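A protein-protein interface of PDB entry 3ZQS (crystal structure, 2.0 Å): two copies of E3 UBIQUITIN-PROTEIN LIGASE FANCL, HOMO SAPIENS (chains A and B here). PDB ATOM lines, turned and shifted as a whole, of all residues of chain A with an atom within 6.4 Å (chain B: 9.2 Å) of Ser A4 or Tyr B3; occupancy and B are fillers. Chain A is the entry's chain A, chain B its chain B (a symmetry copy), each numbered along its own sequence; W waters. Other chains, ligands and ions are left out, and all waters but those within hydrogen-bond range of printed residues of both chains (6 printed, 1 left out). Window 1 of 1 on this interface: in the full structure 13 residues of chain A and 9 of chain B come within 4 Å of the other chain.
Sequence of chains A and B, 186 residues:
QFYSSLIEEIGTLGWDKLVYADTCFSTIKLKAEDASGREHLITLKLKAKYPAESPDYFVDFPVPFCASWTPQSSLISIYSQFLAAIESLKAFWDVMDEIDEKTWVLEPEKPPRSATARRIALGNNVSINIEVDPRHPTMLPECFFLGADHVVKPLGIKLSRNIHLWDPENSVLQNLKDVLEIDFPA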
ATOM      1  N   GLN A   1       8.687  29.984   6.950  1.00  0.00           N
ATOM      2  CA  GLN A   1       7.758  30.151   8.066  1.00  0.00           C
ATOM      3  C   GLN A   1       7.400  28.774   8.643  1.00  0.00           C
ATOM      4  O   GLN A   1       7.154  27.842   7.878  1.00  0.00           O
ATOM      5  CB  GLN A   1       6.487  30.871   7.602  1.00  0.00           C
ATOM      6  CG  GLN A   1       5.654  30.113   6.555  1.00  0.00           C
ATOM      7  CD  GLN A   1       4.270  30.743   6.323  1.00  0.00           C
ATOM      8  OE1 GLN A   1       4.158  31.952   6.100  1.00  0.00           O
ATOM      9  NE2 GLN A   1       3.214  29.922   6.385  1.00  0.00           N
ATOM     10  N   PHE A   2       7.387  28.620   9.969  1.00  0.00           N
ATOM     11  CA  PHE A   2       7.032  27.300  10.512  1.00  0.00           C
ATOM     12  C   PHE A   2       5.525  27.083  10.464  1.00  0.00           C
ATOM     13  O   PHE A   2       5.044  26.094   9.905  1.00  0.00           O
ATOM     14  CB  PHE A   2       7.559  27.081  11.929  1.00  0.00           C
ATOM     15  CG  PHE A   2       7.308  25.681  12.468  1.00  0.00           C
ATOM     16  CD1 PHE A   2       6.060  25.319  12.942  1.00  0.00           C
ATOM     17  CD2 PHE A   2       8.322  24.731  12.488  1.00  0.00           C
ATOM     18  CE1 PHE A   2       5.828  24.044  13.446  1.00  0.00           C
ATOM     19  CE2 PHE A   2       8.101  23.447  12.984  1.00  0.00           C
ATOM     20  CZ  PHE A   2       6.851  23.101  13.462  1.00  0.00           C
ATOM     21  N   TYR A   3       4.777  28.000  11.059  1.00  0.00           N
ATOM     22  CA  TYR A   3       3.326  27.855  11.132  1.00  0.00           C
ATOM     23  C   TYR A   3       2.645  28.281   9.839  1.00  0.00           C
ATOM     24  O   TYR A   3       3.142  29.149   9.134  1.00  0.00           O
ATOM     25  CB  TYR A   3       2.774  28.712  12.270  1.00  0.00           C
ATOM     26  CG  TYR A   3       3.256  28.263  13.620  1.00  0.00           C
ATOM     27  CD1 TYR A   3       2.864  27.035  14.144  1.00  0.00           C
ATOM     28  CD2 TYR A   3       4.127  29.044  14.353  1.00  0.00           C
ATOM     29  CE1 TYR A   3       3.315  26.609  15.375  1.00  0.00           C
ATOM     30  CE2 TYR A   3       4.578  28.635  15.586  1.00  0.00           C
ATOM     31  CZ  TYR A   3       4.171  27.422  16.094  1.00  0.00           C
ATOM     32  OH  TYR A   3       4.632  27.025  17.331  1.00  0.00           O
ATOM     33  N   SER A   4       1.502  27.686   9.528  1.00  0.00           N
ATOM     34  CA  SER A   4       0.685  28.255   8.475  1.00  0.00           C
ATOM     35  C   SER A   4       0.240  29.635   8.916  1.00  0.00           C
ATOM     36  O   SER A   4       0.445  30.076  10.044  1.00  0.00           O
ATOM     37  CB  SER A   4      -0.556  27.402   8.214  1.00  0.00           C
ATOM     38  OG  SER A   4      -1.412  27.434   9.323  1.00  0.00           O
ATOM     39  N   SER A   5      -0.400  30.305   7.992  1.00  0.00           N
ATOM     40  CA  SER A   5      -0.961  31.621   8.149  1.00  0.00           C
ATOM     41  C   SER A   5      -2.467  31.476   8.359  1.00  0.00           C
ATOM     42  O   SER A   5      -3.174  32.479   8.387  1.00  0.00           O
ATOM     43  CB  SER A   5      -0.750  32.407   6.856  1.00  0.00           C
ATOM     44  OG  SER A   5      -1.504  31.820   5.792  1.00  0.00           O
ATOM     45  N   LEU A   6      -2.957  30.242   8.491  1.00  0.00           N
ATOM     46  CA  LEU A   6      -4.397  29.996   8.673  1.00  0.00           C
ATOM     47  C   LEU A   6      -4.923  30.724   9.901  1.00  0.00           C
ATOM     48  O   LEU A   6      -5.951  31.414   9.874  1.00  0.00           O
ATOM     49  CB  LEU A   6      -4.689  28.497   8.790  1.00  0.00           C
ATOM     50  CG  LEU A   6      -6.155  28.101   8.973  1.00  0.00           C
ATOM     51  CD1 LEU A   6      -6.977  28.570   7.778  1.00  0.00           C
ATOM     52  CD2 LEU A   6      -6.263  26.576   9.145  1.00  0.00           C
ATOM     53  N   ILE A   7      -4.190  30.605  10.991  1.00  0.00           N
ATOM     54  CA  ILE A   7      -4.643  31.214  12.225  1.00  0.00           C
ATOM     55  C   ILE A   7      -4.659  32.740  12.152  1.00  0.00           C
ATOM     56  O   ILE A   7      -5.523  33.381  12.728  1.00  0.00           O
ATOM     57  CB  ILE A   7      -3.770  30.767  13.401  1.00  0.00           C
ATOM     58  CG1 ILE A   7      -3.826  29.241  13.516  1.00  0.00           C
ATOM     59  CG2 ILE A   7      -4.241  31.413  14.672  1.00  0.00           C
ATOM     60  CD1 ILE A   7      -5.241  28.669  13.407  1.00  0.00           C
ATOM     61  N   GLU A   8      -3.688  33.320  11.460  1.00  0.00           N
ATOM     62  CA  GLU A   8      -3.647  34.759  11.289  1.00  0.00           C
ATOM     63  C   GLU A   8      -4.839  35.195  10.457  1.00  0.00           C
ATOM     64  O   GLU A   8      -5.494  36.200  10.749  1.00  0.00           O
ATOM     65  CB  GLU A   8      -2.328  35.164  10.616  1.00  0.00           C
ATOM     66  CG  GLU A   8      -2.210  36.651  10.317  1.00  0.00           C
ATOM     67  CD  GLU A   8      -0.894  37.003   9.625  1.00  0.00           C
ATOM     68  OE1 GLU A   8      -0.664  36.528   8.487  1.00  0.00           O
ATOM     69  OE2 GLU A   8      -0.092  37.756  10.223  1.00  0.00           O
ATOM     70  N   CYS A  24      -6.906  19.388  14.497  1.00  0.00           N
ATOM     71  CA  CYS A  24      -5.739  19.788  13.709  1.00  0.00           C
ATOM     72  C   CYS A  24      -6.020  20.994  12.823  1.00  0.00           C
ATOM     73  O   CYS A  24      -5.179  21.397  12.043  1.00  0.00           O
ATOM     74  CB  CYS A  24      -5.262  18.627  12.828  1.00  0.00           C
ATOM     75  SG  CYS A  24      -5.052  17.051  13.684  1.00  0.00           S
ATOM     76  N   LYS A  47      -5.243  21.520   3.414  1.00  0.00           N
ATOM     77  CA  LYS A  47      -4.039  20.703   3.480  1.00  0.00           C
ATOM     78  C   LYS A  47      -2.844  21.551   3.898  1.00  0.00           C
ATOM     79  O   LYS A  47      -2.908  22.784   3.828  1.00  0.00           O
ATOM     80  CB  LYS A  47      -3.783  20.044   2.128  1.00  0.00           C
ATOM     81  CG  LYS A  47      -4.740  18.905   1.833  1.00  0.00           C
ATOM     82  CD  LYS A  47      -4.538  18.373   0.422  1.00  0.00           C
ATOM     83  CE  LYS A  47      -5.661  17.426   0.018  1.00  0.00           C
ATOM     84  NZ  LYS A  47      -5.618  17.098  -1.437  1.00  0.00           N
ATOM     85  N   ALA A  48      -1.752  20.900   4.316  1.00  0.00           N
ATOM     86  CA  ALA A  48      -0.539  21.618   4.713  1.00  0.00           C
ATOM     87  C   ALA A  48      -0.023  22.533   3.602  1.00  0.00           C
ATOM     88  O   ALA A  48       0.605  23.559   3.872  1.00  0.00           O
ATOM     89  CB  ALA A  48       0.545  20.646   5.140  1.00  0.00           C
ATOM     90  N   LYS A  49      -0.310  22.169   2.355  1.00  0.00           N
ATOM     91  CA  LYS A  49       0.137  22.942   1.188  1.00  0.00           C
ATOM     92  C   LYS A  49      -0.675  24.219   0.978  1.00  0.00           C
ATOM     93  O   LYS A  49      -0.404  25.010   0.068  1.00  0.00           O
ATOM     94  CB  LYS A  49       0.100  22.072  -0.074  1.00  0.00           C
ATOM     95  CG  LYS A  49       1.194  21.005  -0.125  1.00  0.00           C
ATOM     96  CD  LYS A  49       1.077  20.167  -1.392  1.00  0.00           C
ATOM     97  CE  LYS A  49       2.308  19.297  -1.612  1.00  0.00           C
ATOM     98  NZ  LYS A  49       2.393  18.809  -3.027  1.00  0.00           N
ATOM     99  N   TYR A  50      -1.682  24.421   1.815  1.00  0.00           N
ATOM    100  CA  TYR A  50      -2.366  25.708   1.865  1.00  0.00           C
ATOM    101  C   TYR A  50      -1.354  26.825   2.129  1.00  0.00           C
ATOM    102  O   TYR A  50      -0.492  26.680   2.990  1.00  0.00           O
ATOM    103  CB  TYR A  50      -3.385  25.681   2.995  1.00  0.00           C
ATOM    104  CG  TYR A  50      -4.145  26.969   3.178  1.00  0.00           C
ATOM    105  CD1 TYR A  50      -3.651  27.977   3.985  1.00  0.00           C
ATOM    106  CD2 TYR A  50      -5.367  27.166   2.551  1.00  0.00           C
ATOM    107  CE1 TYR A  50      -4.346  29.155   4.152  1.00  0.00           C
ATOM    108  CE2 TYR A  50      -6.074  28.336   2.723  1.00  0.00           C
ATOM    109  CZ  TYR A  50      -5.551  29.327   3.517  1.00  0.00           C
ATOM    110  OH  TYR A  50      -6.248  30.494   3.686  1.00  0.00           O
ATOM    111  N   GLN B   1      -4.270  23.202   8.561  1.00  0.00           N
ATOM    112  CA  GLN B   1      -3.257  22.632   9.450  1.00  0.00           C
ATOM    113  C   GLN B   1      -2.535  23.762  10.148  1.00  0.00           C
ATOM    114  O   GLN B   1      -2.582  24.905   9.696  1.00  0.00           O
ATOM    115  CB  GLN B   1      -2.263  21.757   8.666  1.00  0.00           C
ATOM    116  CG  GLN B   1      -2.747  20.318   8.397  1.00  0.00           C
ATOM    117  CD  GLN B   1      -3.855  20.217   7.339  1.00  0.00           C
ATOM    118  OE1 GLN B   1      -4.256  19.114   6.952  1.00  0.00           O
ATOM    119  NE2 GLN B   1      -4.344  21.360   6.867  1.00  0.00           N
ATOM    120  N   PHE B   2      -1.868  23.460  11.254  1.00  0.00           N
ATOM    121  CA  PHE B   2      -1.115  24.507  11.932  1.00  0.00           C
ATOM    122  C   PHE B   2       0.241  24.825  11.293  1.00  0.00           C
ATOM    123  O   PHE B   2       0.812  25.873  11.588  1.00  0.00           O
ATOM    124  CB  PHE B   2      -0.891  24.170  13.407  1.00  0.00           C
ATOM    125  CG  PHE B   2      -2.144  23.936  14.185  1.00  0.00           C
ATOM    126  CD1 PHE B   2      -2.997  24.983  14.503  1.00  0.00           C
ATOM    127  CD2 PHE B   2      -2.459  22.669  14.634  1.00  0.00           C
ATOM    128  CE1 PHE B   2      -4.132  24.757  15.226  1.00  0.00           C
ATOM    129  CE2 PHE B   2      -3.591  22.441  15.370  1.00  0.00           C
ATOM    130  CZ  PHE B   2      -4.439  23.481  15.664  1.00  0.00           C
ATOM    131  N   TYR B   3       0.763  23.932  10.444  1.00  0.00           N
ATOM    132  CA  TYR B   3       2.117  24.071   9.881  1.00  0.00           C
ATOM    133  C   TYR B   3       2.115  24.340   8.361  1.00  0.00           C
ATOM    134  O   TYR B   3       1.141  24.026   7.670  1.00  0.00           O
ATOM    135  CB  TYR B   3       2.972  22.823  10.213  1.00  0.00           C
ATOM    136  CG  TYR B   3       2.269  21.527   9.878  1.00  0.00           C
ATOM    137  CD1 TYR B   3       1.412  20.918  10.798  1.00  0.00           C
ATOM    138  CD2 TYR B   3       2.422  20.932   8.637  1.00  0.00           C
ATOM    139  CE1 TYR B   3       0.739  19.757  10.486  1.00  0.00           C
ATOM    140  CE2 TYR B   3       1.760  19.758   8.315  1.00  0.00           C
ATOM    141  CZ  TYR B   3       0.920  19.181   9.237  1.00  0.00           C
ATOM    142  OH  TYR B   3       0.254  18.023   8.907  1.00  0.00           O
ATOM    143  N   SER B   4       3.203  24.928   7.861  1.00  0.00           N
ATOM    144  CA  SER B   4       3.371  25.333   6.439  1.00  0.00           C
ATOM    145  C   SER B   4       3.779  24.173   5.518  1.00  0.00           C
ATOM    146  O   SER B   4       4.134  23.115   6.053  1.00  0.00           O
ATOM    147  CB  SER B   4       4.460  26.393   6.376  1.00  0.00           C
ATOM    148  OG  SER B   4       5.687  25.857   6.867  1.00  0.00           O
ATOM    149  N   SER B   5       3.776  24.317   4.168  1.00  0.00           N
ATOM    150  CA  SER B   5       4.140  23.178   3.337  1.00  0.00           C
ATOM    151  C   SER B   5       5.581  22.775   3.648  1.00  0.00           C
ATOM    152  O   SER B   5       5.968  21.607   3.508  1.00  0.00           O
ATOM    153  CB  SER B   5       3.961  23.491   1.847  1.00  0.00           C
ATOM    154  OG  SER B   5       3.959  24.889   1.610  1.00  0.00           O
ATOM    155  N   LEU B   6       6.374  23.747   4.089  1.00  0.00           N
ATOM    156  CA  LEU B   6       7.794  23.496   4.362  1.00  0.00           C
ATOM    157  C   LEU B   6       7.933  22.480   5.480  1.00  0.00           C
ATOM    158  O   LEU B   6       8.709  21.547   5.378  1.00  0.00           O
ATOM    159  CB  LEU B   6       8.500  24.794   4.753  1.00  0.00           C
ATOM    160  CG  LEU B   6       9.973  24.686   5.149  1.00  0.00           C
ATOM    161  CD1 LEU B   6      10.792  24.177   3.970  1.00  0.00           C
ATOM    162  CD2 LEU B   6      10.506  26.034   5.627  1.00  0.00           C
ATOM    163  N   ILE B   7       7.147  22.649   6.535  1.00  0.00           N
ATOM    164  CA  ILE B   7       7.224  21.752   7.668  1.00  0.00           C
ATOM    165  C   ILE B   7       6.792  20.341   7.278  1.00  0.00           C
ATOM    166  O   ILE B   7       7.341  19.356   7.762  1.00  0.00           O
ATOM    167  CB  ILE B   7       6.356  22.278   8.828  1.00  0.00           C
ATOM    168  CG1 ILE B   7       6.826  23.682   9.211  1.00  0.00           C
ATOM    169  CG2 ILE B   7       6.442  21.336  10.012  1.00  0.00           C
ATOM    170  CD1 ILE B   7       8.329  23.798   9.351  1.00  0.00           C
ATOM    171  N   GLU B   8       5.792  20.231   6.413  1.00  0.00           N
ATOM    172  CA  GLU B   8       5.356  18.908   5.978  1.00  0.00           C
ATOM    173  C   GLU B   8       6.469  18.247   5.164  1.00  0.00           C
ATOM    174  O   GLU B   8       6.769  17.065   5.357  1.00  0.00           O
ATOM    175  CB  GLU B   8       4.076  19.005   5.150  1.00  0.00           C
ATOM    176  CG  GLU B   8       3.544  17.665   4.683  1.00  0.00           C
ATOM    177  CD  GLU B   8       2.276  17.813   3.868  1.00  0.00           C
ATOM    178  OE1 GLU B   8       2.320  18.471   2.812  1.00  0.00           O
ATOM    179  OE2 GLU B   8       1.230  17.275   4.283  1.00  0.00           O
ATOM    180  N   GLU B   9       7.102  19.018   4.263  1.00  0.00           N
ATOM    181  CA  GLU B   9       8.290  18.531   3.536  1.00  0.00           C
ATOM    182  C   GLU B   9       9.434  18.067   4.440  1.00  0.00           C
ATOM    183  O   GLU B   9      10.035  17.024   4.176  1.00  0.00           O
ATOM    184  CB  GLU B   9       8.793  19.564   2.514  1.00  0.00           C
ATOM    185  CG  GLU B   9       7.748  19.839   1.420  1.00  0.00           C
ATOM    186  CD  GLU B   9       8.056  21.080   0.610  1.00  0.00           C
ATOM    187  OE1 GLU B   9       9.234  21.293   0.319  1.00  0.00           O
ATOM    188  OE2 GLU B   9       7.123  21.843   0.258  1.00  0.00           O
ATOM    189  N   ILE B  10       9.733  18.812   5.503  1.00  0.00           N
ATOM    190  CA  ILE B  10      10.832  18.411   6.383  1.00  0.00           C
ATOM    191  C   ILE B  10      10.459  17.113   7.080  1.00  0.00           C
ATOM    192  O   ILE B  10      11.292  16.229   7.216  1.00  0.00           O
ATOM    193  CB  ILE B  10      11.184  19.497   7.422  1.00  0.00           C
ATOM    194  CG1 ILE B  10      11.828  20.696   6.724  1.00  0.00           C
ATOM    195  CG2 ILE B  10      12.130  18.931   8.497  1.00  0.00           C
ATOM    196  CD1 ILE B  10      12.007  21.908   7.621  1.00  0.00           C
ATOM    197  N   GLY B  11       9.201  16.989   7.506  1.00  0.00           N
ATOM    198  CA  GLY B  11       8.738  15.771   8.159  1.00  0.00           C
ATOM    199  C   GLY B  11       8.874  14.551   7.265  1.00  0.00           C
ATOM    200  O   GLY B  11       9.194  13.447   7.717  1.00  0.00           O
ATOM    201  N   THR B  12       8.612  14.749   5.980  1.00  0.00           N
ATOM    202  CA  THR B  12       8.775  13.690   4.992  1.00  0.00           C
ATOM    203  C   THR B  12      10.243  13.276   4.799  1.00  0.00           C
ATOM    204  O   THR B  12      10.548  12.096   4.722  1.00  0.00           O
ATOM    205  CB  THR B  12       8.213  14.112   3.630  1.00  0.00           C
ATOM    206  OG1 THR B  12       6.814  14.390   3.749  1.00  0.00           O
ATOM    207  CG2 THR B  12       8.408  12.998   2.618  1.00  0.00           C
ATOM    208  N   TRP B  15      13.087  14.556  10.370  1.00  0.00           N
ATOM    209  CA  TRP B  15      13.628  15.636  11.175  1.00  0.00           C
ATOM    210  C   TRP B  15      15.100  15.424  11.465  1.00  0.00           C
ATOM    211  O   TRP B  15      15.811  16.389  11.689  1.00  0.00           O
ATOM    212  CB  TRP B  15      12.794  15.836  12.443  1.00  0.00           C
ATOM    213  CG  TRP B  15      11.473  16.441  12.101  1.00  0.00           C
ATOM    214  CD1 TRP B  15      10.303  15.780  11.868  1.00  0.00           C
ATOM    215  CD2 TRP B  15      11.193  17.833  11.899  1.00  0.00           C
ATOM    216  NE1 TRP B  15       9.308  16.675  11.553  1.00  0.00           N
ATOM    217  CE2 TRP B  15       9.832  17.940  11.558  1.00  0.00           C
ATOM    218  CE3 TRP B  15      11.965  18.999  11.971  1.00  0.00           C
ATOM    219  CZ2 TRP B  15       9.218  19.165  11.311  1.00  0.00           C
ATOM    220  CZ3 TRP B  15      11.360  20.214  11.714  1.00  0.00           C
ATOM    221  CH2 TRP B  15       9.999  20.288  11.393  1.00  0.00           C
HETATM  222  O   HOH W   1       2.396  26.439   3.368  1.00  0.00           O
HETATM  223  O   HOH W   2      -2.371  20.915  11.885  1.00  0.00           O
HETATM  224  O   HOH W   3      -0.412  19.108   1.841  1.00  0.00           O
HETATM  225  O   HOH W   4      -3.091  24.596   6.498  1.00  0.00           O
HETATM  226  O   HOH W   5       2.411  24.864  -0.658  1.00  0.00           O
HETATM  227  O   HOH W   6      -1.412  18.263   4.554  1.00  0.00           O
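O of Gln A1 is in hydrogen-bond range of OG of Ser B4 (2.7 Å).
The side-chain hydroxyl (OG) of Ser A4 sits at hydrogen-bond distance from the backbone carbonyl oxygen (O) of Gln B1, 2.8 Å away.
The backbone carbonyl oxygen of Phe A2 lies within hydrogen-bond range of the backbone NH of Ser B4.
N of Ser B5 sits at hydrogen-bond distance from O of Ala A48 (3.3 Å).
The backbone NH of Ser A4 is in hydrogen-bond range of the backbone carbonyl oxygen of Phe B2.
The side-chain hydroxyl of Thr B12 is in hydrogen-bond range of the backbone carbonyl oxygen of Glu B8, at 3.1 Å.
NE2 of Gln A1 lies within hydrogen-bond range of O of Tyr A3, at 2.9 Å.
The side-chain hydroxyl (OG) of Ser A4 lies close to the backbone NH (N) of Leu A6, 3.3 Å away.
Among the printed residues, merely in contact across the chains: Phe A2 with Tyr B3 (3.6 Å), Phe A2 with Ile B7 (3.1 Å), Tyr A3 with Phe B2 (3.2 Å), Tyr A3 with Ser B4 (3.9 Å), Ser A4 with Tyr B3 (3.6 Å), Ser A4 with Ser B4 (3.6 Å), Leu A6 with Gln B1 (3.96 Å), Cys A24 with Gln B1 (3.5 Å), Cys A24 with Phe B2 (3.8 Å), Lys A47 with Gln B1 (3.3 Å), Ala A48 with Gln B1 (3.7 Å), Ala A48 with Tyr B3 (3.5 Å), Ala A48 with Ser B4 (3.6 Å), Ala A48 with Glu B8 (3.5 Å) and Lys A49 with Ser B5 (3.9 Å).
Printed residues of chain B within 4 Å of Gln A1: Ser B4.
Ser A4 touches just these residues of chain B: Gln B1, Phe B2, Tyr B3 and Ser B4.
Ser A5 touches none of the printed residues of chain B.
Tyr B3 touches just these residues of chain A: Phe A2 (3.6 Å), Ser A4 (3.6 Å) and Ala A48 (3.5 Å).
Printed residues of chain A within 4 Å of Ser B5: Ala A48 (3.3 Å) and Lys A49 (3.9 Å).
Hydrophobic or aromatic side chains of chain A that line the printed part of chain B: Phe A2, Tyr A3, Leu A6 and Ala A48.
Hydrophobic or aromatic side chains of chain B that line the printed part of chain A: Phe B2, Tyr B3 and Ile B7.
Among the printed residues, 20 pairs touch across the chains.
Among the printed residues, no Asp or Glu carboxylate lies within 4 Å of a Lys or Arg side-chain nitrogen of the other chain.
Phe A2 touches Tyr B3, and with the chains exchanged Tyr A3 touches Phe B2.
Phe A2 touches Ser B4, and with the chains exchanged Ser A4 touches Phe B2.
Ser A4 touches its own counterpart, Ser B4.
Leu A6 touches Gln B1, but with the chains exchanged Gln A1 does not touch Leu B6 (4.4 Å).
Water W1 lies within hydrogen-bond range of the backbone NH (N) of Ser B5 (2.7 Å), the backbone carbonyl oxygen (O) of Tyr A50 (2.9 Å) and the backbone carbonyl oxygen (O) of Ala A48 (3.4 Å).
Water W6 bridges the backbone NH of Ala A48 (2.7 Å) and the side-chain carboxylate of Glu B8 (2.8 Å).
Water W2 lies within hydrogen-bond range of the backbone NH of Phe B2 (2.7 Å) and the backbone carbonyl oxygen of Cys A24 (2.9 Å).
Water W5 lies within hydrogen-bond range of OG of Ser B5 (2.7 Å) and O of Lys A49 (2.9 Å).
Water W4 lies within hydrogen-bond range of the backbone NH of Gln B1 and the backbone carbonyl oxygen of Lys A47.
Water W3 lies within hydrogen-bond range of the side-chain carboxylate (OE1) of Glu B8, the backbone NH (N) of Lys A49 and the backbone NH (N) of Ala A48.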
